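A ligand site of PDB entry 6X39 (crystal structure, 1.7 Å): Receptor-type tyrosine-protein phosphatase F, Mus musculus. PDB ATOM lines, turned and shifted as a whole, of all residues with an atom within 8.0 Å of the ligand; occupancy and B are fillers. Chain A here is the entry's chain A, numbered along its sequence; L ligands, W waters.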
ATOM      1  N   VAL A  46     -25.563  18.125  -8.683  1.00  0.00           N
ATOM      2  CA  VAL A  46     -24.861  16.870  -8.467  1.00  0.00           C
ATOM      3  C   VAL A  46     -24.166  16.966  -7.122  1.00  0.00           C
ATOM      4  O   VAL A  46     -23.664  18.038  -6.749  1.00  0.00           O
ATOM      5  CB  VAL A  46     -23.872  16.553  -9.596  1.00  0.00           C
ATOM      6  CG1 VAL A  46     -22.749  17.543  -9.677  1.00  0.00           C
ATOM      7  CG2 VAL A  46     -23.354  15.084  -9.498  1.00  0.00           C
ATOM      8  N   ARG A  47     -24.234  15.856  -6.377  1.00  0.00           N
ATOM      9  CA  ARG A  47     -23.474  15.748  -5.140  1.00  0.00           C
ATOM     10  C   ARG A  47     -21.980  15.772  -5.465  1.00  0.00           C
ATOM     11  O   ARG A  47     -21.532  15.156  -6.442  1.00  0.00           O
ATOM     12  CB  ARG A  47     -23.809  14.425  -4.440  1.00  0.00           C
ATOM     13  CG  ARG A  47     -22.947  14.135  -3.256  1.00  0.00           C
ATOM     14  CD  ARG A  47     -23.441  12.943  -2.451  1.00  0.00           C
ATOM     15  NE  ARG A  47     -22.418  12.628  -1.476  1.00  0.00           N
ATOM     16  CZ  ARG A  47     -21.459  11.726  -1.666  1.00  0.00           C
ATOM     17  NH1 ARG A  47     -21.445  10.965  -2.785  1.00  0.00           N
ATOM     18  NH2 ARG A  47     -20.548  11.517  -0.715  1.00  0.00           N
ATOM     19  N   LEU A  48     -21.219  16.463  -4.622  1.00  0.00           N
ATOM     20  CA  LEU A  48     -19.775  16.408  -4.662  1.00  0.00           C
ATOM     21  C   LEU A  48     -19.267  15.691  -3.447  1.00  0.00           C
ATOM     22  O   LEU A  48     -19.811  15.825  -2.355  1.00  0.00           O
ATOM     23  CB  LEU A  48     -19.117  17.803  -4.661  1.00  0.00           C
ATOM     24  CG  LEU A  48     -19.489  18.780  -5.752  1.00  0.00           C
ATOM     25  CD1 LEU A  48     -18.647  20.016  -5.584  1.00  0.00           C
ATOM     26  CD2 LEU A  48     -19.311  18.209  -7.081  1.00  0.00           C
ATOM     27  N   GLU A  49     -18.197  14.925  -3.643  1.00  0.00           N
ATOM     28  CA  GLU A  49     -17.487  14.289  -2.555  1.00  0.00           C
ATOM     29  C   GLU A  49     -16.026  14.700  -2.702  1.00  0.00           C
ATOM     30  O   GLU A  49     -15.374  14.348  -3.686  1.00  0.00           O
ATOM     31  CB  GLU A  49     -17.664  12.764  -2.638  1.00  0.00           C
ATOM     32  CG  GLU A  49     -16.994  11.967  -1.565  1.00  0.00           C
ATOM     33  CD  GLU A  49     -17.152  10.488  -1.876  1.00  0.00           C
ATOM     34  OE1 GLU A  49     -16.386   9.970  -2.729  1.00  0.00           O
ATOM     35  OE2 GLU A  49     -18.075   9.864  -1.295  1.00  0.00           O
ATOM     36  N   ASN A  50     -15.539  15.444  -1.722  1.00  0.00           N
ATOM     37  CA  ASN A  50     -14.182  15.991  -1.758  1.00  0.00           C
ATOM     38  C   ASN A  50     -13.946  16.704  -3.079  1.00  0.00           C
ATOM     39  O   ASN A  50     -12.871  16.642  -3.668  1.00  0.00           O
ATOM     40  CB  ASN A  50     -13.188  14.882  -1.500  1.00  0.00           C
ATOM     41  CG  ASN A  50     -13.388  14.271  -0.137  1.00  0.00           C
ATOM     42  OD1 ASN A  50     -13.742  14.976   0.824  1.00  0.00           O
ATOM     43  ND2 ASN A  50     -13.201  12.955  -0.035  1.00  0.00           N
ATOM     44  N   GLY A  51     -14.982  17.437  -3.537  1.00  0.00           N
ATOM     45  CA  GLY A  51     -14.893  18.276  -4.705  1.00  0.00           C
ATOM     46  C   GLY A  51     -15.162  17.578  -6.005  1.00  0.00           C
ATOM     47  O   GLY A  51     -15.211  18.228  -7.042  1.00  0.00           O
ATOM     48  N   GLU A  52     -15.353  16.233  -5.985  1.00  0.00           N
ATOM     49  CA  GLU A  52     -15.600  15.450  -7.185  1.00  0.00           C
ATOM     50  C   GLU A  52     -17.081  15.104  -7.317  1.00  0.00           C
ATOM     51  O   GLU A  52     -17.697  14.667  -6.351  1.00  0.00           O
ATOM     52  CB  GLU A  52     -14.812  14.135  -7.131  1.00  0.00           C
ATOM     53  CG  GLU A  52     -13.369  14.295  -6.747  1.00  0.00           C
ATOM     54  CD  GLU A  52     -12.568  15.042  -7.773  1.00  0.00           C
ATOM     55  OE1 GLU A  52     -13.033  15.109  -8.933  1.00  0.00           O
ATOM     56  OE2 GLU A  52     -11.463  15.553  -7.427  1.00  0.00           O
ATOM     57  N   ARG A  54     -20.316  12.966  -7.757  1.00  0.00           N
ATOM     58  CA  ARG A  54     -20.573  11.540  -7.531  1.00  0.00           C
ATOM     59  C   ARG A  54     -22.059  11.296  -7.705  1.00  0.00           C
ATOM     60  O   ARG A  54     -22.873  12.040  -7.130  1.00  0.00           O
ATOM     61  CB  ARG A  54     -20.140  11.119  -6.136  1.00  0.00           C
ATOM     62  CG  ARG A  54     -18.627  11.110  -5.930  1.00  0.00           C
ATOM     63  CD  ARG A  54     -17.976   9.977  -6.685  1.00  0.00           C
ATOM     64  NE  ARG A  54     -18.376   8.697  -6.109  1.00  0.00           N
ATOM     65  CZ  ARG A  54     -18.008   7.545  -6.638  1.00  0.00           C
ATOM     66  NH1 ARG A  54     -17.260   7.544  -7.718  1.00  0.00           N
ATOM     67  NH2 ARG A  54     -18.409   6.428  -6.078  1.00  0.00           N
ATOM     68  N   THR A  76     -29.758  15.761   0.970  1.00  0.00           N
ATOM     69  CA  THR A  76     -29.335  15.139   2.215  1.00  0.00           C
ATOM     70  C   THR A  76     -28.584  16.155   3.079  1.00  0.00           C
ATOM     71  O   THR A  76     -27.828  16.991   2.549  1.00  0.00           O
ATOM     72  CB  THR A  76     -28.458  13.891   1.941  1.00  0.00           C
ATOM     73  OG1 THR A  76     -27.377  14.208   1.043  1.00  0.00           O
ATOM     74  CG2 THR A  76     -29.257  12.826   1.322  1.00  0.00           C
ATOM     75  N   PRO A  77     -28.781  16.141   4.402  1.00  0.00           N
ATOM     76  CA  PRO A  77     -28.068  17.090   5.270  1.00  0.00           C
ATOM     77  C   PRO A  77     -26.559  16.934   5.205  1.00  0.00           C
ATOM     78  O   PRO A  77     -26.031  15.855   4.932  1.00  0.00           O
ATOM     79  CB  PRO A  77     -28.588  16.745   6.686  1.00  0.00           C
ATOM     80  CG  PRO A  77     -29.906  16.110   6.445  1.00  0.00           C
ATOM     81  CD  PRO A  77     -29.788  15.350   5.155  1.00  0.00           C
ATOM     82  N   GLU A  78     -25.867  18.009   5.500  1.00  0.00           N
ATOM     83  CA  GLU A  78     -24.411  18.006   5.555  1.00  0.00           C
ATOM     84  C   GLU A  78     -23.819  17.417   4.285  1.00  0.00           C
ATOM     85  O   GLU A  78     -22.920  16.580   4.333  1.00  0.00           O
ATOM     86  CB  GLU A  78     -23.913  17.231   6.777  1.00  0.00           C
ATOM     87  CG  GLU A  78     -24.210  17.903   8.094  1.00  0.00           C
ATOM     88  CD  GLU A  78     -23.717  17.090   9.273  1.00  0.00           C
ATOM     89  OE1 GLU A  78     -23.296  15.931   9.071  1.00  0.00           O
ATOM     90  OE2 GLU A  78     -23.754  17.606  10.406  1.00  0.00           O
ATOM     91  N   THR A  79     -24.365  17.818   3.144  1.00  0.00           N
ATOM     92  CA  THR A  79     -23.977  17.292   1.848  1.00  0.00           C
ATOM     93  C   THR A  79     -23.730  18.438   0.885  1.00  0.00           C
ATOM     94  O   THR A  79     -24.456  19.452   0.892  1.00  0.00           O
ATOM     95  CB  THR A  79     -25.044  16.344   1.256  1.00  0.00           C
ATOM     96  OG1 THR A  79     -25.301  15.279   2.167  1.00  0.00           O
ATOM     97  CG2 THR A  79     -24.595  15.787  -0.109  1.00  0.00           C
ATOM     98  N   THR A  80     -22.700  18.273   0.060  1.00  0.00           N
ATOM     99  CA  THR A  80     -22.243  19.292  -0.864  1.00  0.00           C
ATOM    100  C   THR A  80     -22.825  19.049  -2.251  1.00  0.00           C
ATOM    101  O   THR A  80     -22.810  17.929  -2.739  1.00  0.00           O
ATOM    102  CB  THR A  80     -20.724  19.319  -0.916  1.00  0.00           C
ATOM    103  OG1 THR A  80     -20.207  19.497   0.409  1.00  0.00           O
ATOM    104  CG2 THR A  80     -20.168  20.426  -1.785  1.00  0.00           C
ATOM    105  N   TYR A  81     -23.311  20.130  -2.879  1.00  0.00           N
ATOM    106  CA  TYR A  81     -23.947  20.062  -4.205  1.00  0.00           C
ATOM    107  C   TYR A  81     -23.413  21.146  -5.112  1.00  0.00           C
ATOM    108  O   TYR A  81     -23.243  22.310  -4.697  1.00  0.00           O
ATOM    109  CB  TYR A  81     -25.482  20.191  -4.104  1.00  0.00           C
ATOM    110  CG  TYR A  81     -26.126  19.091  -3.378  1.00  0.00           C
ATOM    111  CD1 TYR A  81     -26.434  17.883  -3.999  1.00  0.00           C
ATOM    112  CD2 TYR A  81     -26.375  19.180  -2.012  1.00  0.00           C
ATOM    113  CE1 TYR A  81     -27.027  16.851  -3.321  1.00  0.00           C
ATOM    114  CE2 TYR A  81     -26.972  18.135  -1.324  1.00  0.00           C
ATOM    115  CZ  TYR A  81     -27.272  16.969  -1.985  1.00  0.00           C
ATOM    116  OH  TYR A  81     -27.859  15.919  -1.310  1.00  0.00           O
ATOM    117  N   VAL A 101     -21.513  26.120  -5.713  1.00  0.00           N
ATOM    118  CA  VAL A 101     -21.416  24.968  -4.837  1.00  0.00           C
ATOM    119  C   VAL A 101     -21.797  25.370  -3.430  1.00  0.00           C
ATOM    120  O   VAL A 101     -21.275  26.358  -2.914  1.00  0.00           O
ATOM    121  CB  VAL A 101     -19.984  24.367  -4.840  1.00  0.00           C
ATOM    122  CG1 VAL A 101     -19.951  23.184  -3.910  1.00  0.00           C
ATOM    123  CG2 VAL A 101     -19.574  23.952  -6.235  1.00  0.00           C
ATOM    124  N   VAL A 102     -22.709  24.593  -2.814  1.00  0.00           N
ATOM    125  CA  VAL A 102     -23.181  24.825  -1.471  1.00  0.00           C
ATOM    126  C   VAL A 102     -23.201  23.521  -0.694  1.00  0.00           C
ATOM    127  O   VAL A 102     -23.231  22.436  -1.282  1.00  0.00           O
ATOM    128  CB  VAL A 102     -24.598  25.497  -1.476  1.00  0.00           C
ATOM    129  CG1 VAL A 102     -24.561  26.825  -2.183  1.00  0.00           C
ATOM    130  CG2 VAL A 102     -25.613  24.546  -2.133  1.00  0.00           C
ATOM    131  N   THR A 103     -23.145  23.617   0.626  1.00  0.00           N
ATOM    132  CA  THR A 103     -23.272  22.452   1.506  1.00  0.00           C
ATOM    133  C   THR A 103     -24.416  22.681   2.469  1.00  0.00           C
ATOM    134  O   THR A 103     -24.512  23.748   3.097  1.00  0.00           O
ATOM    135  CB  THR A 103     -21.951  22.164   2.242  1.00  0.00           C
ATOM    136  OG1 THR A 103     -20.939  21.980   1.254  1.00  0.00           O
ATOM    137  CG2 THR A 103     -22.027  20.927   3.081  1.00  0.00           C
ATOM    138  N   THR A 104     -25.346  21.725   2.494  1.00  0.00           N
ATOM    139  CA  THR A 104     -26.502  21.824   3.376  1.00  0.00           C
ATOM    140  C   THR A 104     -26.071  21.742   4.854  1.00  0.00           C
ATOM    141  O   THR A 104     -25.038  21.156   5.202  1.00  0.00           O
ATOM    142  CB  THR A 104     -27.517  20.735   3.079  1.00  0.00           C
ATOM    143  OG1 THR A 104     -26.870  19.469   3.069  1.00  0.00           O
ATOM    144  CG2 THR A 104     -28.161  20.919   1.705  1.00  0.00           C
HETATM  145  C1  LIG L   1     -17.626  18.146   1.599  1.00  0.00           C
HETATM  146  C2  LIG L   1     -17.826  16.625   1.626  1.00  0.00           C
HETATM  147  C3  LIG L   1     -19.320  16.322   2.009  1.00  0.00           C
HETATM  148  C4  LIG L   1     -20.072  15.336   1.095  1.00  0.00           C
HETATM  149  C5  LIG L   1     -20.924  14.534   2.088  1.00  0.00           C
HETATM  150  C6  LIG L   1     -21.769  13.533   1.321  1.00  0.00           C
HETATM  151  O1  LIG L   1     -16.463  18.658   0.968  1.00  0.00           O
HETATM  152  O2  LIG L   1     -17.281  15.960   0.506  1.00  0.00           O
HETATM  153  O3  LIG L   1     -20.127  17.505   2.238  1.00  0.00           O
HETATM  154  O4  LIG L   1     -20.881  15.965   0.094  1.00  0.00           O
HETATM  155  O5  LIG L   1     -20.168  13.756   2.985  1.00  0.00           O
HETATM  156  O6  LIG L   1     -21.662  12.292   1.937  1.00  0.00           O
HETATM  157  O   HOH W   1     -19.860  18.051   4.809  1.00  0.00           O
HETATM  158  O   HOH W   2     -15.956  14.442   2.559  1.00  0.00           O
HETATM  159  O   HOH W   3     -14.083  17.558   1.683  1.00  0.00           O
HETATM  160  O   HOH W   4     -20.992  10.022   2.431  1.00  0.00           O
HETATM  161  O   HOH W   5     -22.326  14.344   5.636  1.00  0.00           O
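An oxygen (O4) of the ligand is in hydrogen-bond range of the backbone carbonyl oxygen (O) of Leu 48, 2.7 Å away.
An oxygen (O4) of the ligand sits at hydrogen-bond distance from the backbone NH of Thr 80, at 2.9 Å.
The side-chain hydroxyl of Thr 80 lies within hydrogen-bond range of an oxygen (O3) of the ligand, at 2.7 Å.
The backbone NH of Asn 50 is in hydrogen-bond range of an oxygen (O2) of the ligand, 2.9 Å away.
O6 of the ligand lies within hydrogen-bond range of NH2 of Arg 47 (3.0 Å).
The backbone NH (N) of Leu 48 lies within hydrogen-bond range of the backbone carbonyl oxygen (O) of Thr 80 (2.9 Å).
The side-chain hydroxyl (OG1) of Thr 80 is in hydrogen-bond range of the side-chain hydroxyl (OG1) of Thr 103, 2.7 Å away.
The guanidinium group (NH2) of Arg 47 lies within salt-bridge range of the side-chain carboxylate (OE2) of Glu 49 (3.0 Å).
The backbone carbonyl oxygen of Arg 47 is in hydrogen-bond range of the backbone NH of Arg 54, 2.8 Å away.
The side-chain hydroxyl (OG1) of Thr 104 sits at hydrogen-bond distance from the backbone NH (N) of Glu 78 (3.0 Å).
The side-chain hydroxyl of Thr 79 is in hydrogen-bond range of the side-chain hydroxyl of Thr 76 (2.6 Å).
O of Pro 77 sits at hydrogen-bond distance from OG1 of Thr 79 (2.9 Å).
O of Thr 79 is in hydrogen-bond range of N of Thr 104, 2.9 Å away.
Glu 49 touches the ligand.
O of Glu 78 touches O3 of the ligand, at 3.6 Å.
CG2 of Thr 79 touches O4 of the ligand, 3.7 Å away.
Within 4 Å of the ligand: Arg 47, Leu 48, Glu 49, Asn 50, Glu 78, Thr 79 and Thr 80.
Water W1 bridges O3 of the ligand and O of Glu 78.
Water W3 bridges an oxygen (O1) of the ligand (2.7 Å) and the side-chain amide oxygen of Asn 50 (2.7 Å).
Water W2 bridges the side-chain amide oxygen (OD1) of Asn 50 and an oxygen (O2) of the ligand.
Water W5 lies within hydrogen-bond range of O of Glu 78 (2.7 Å) and O5 of the ligand (3.5 Å).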
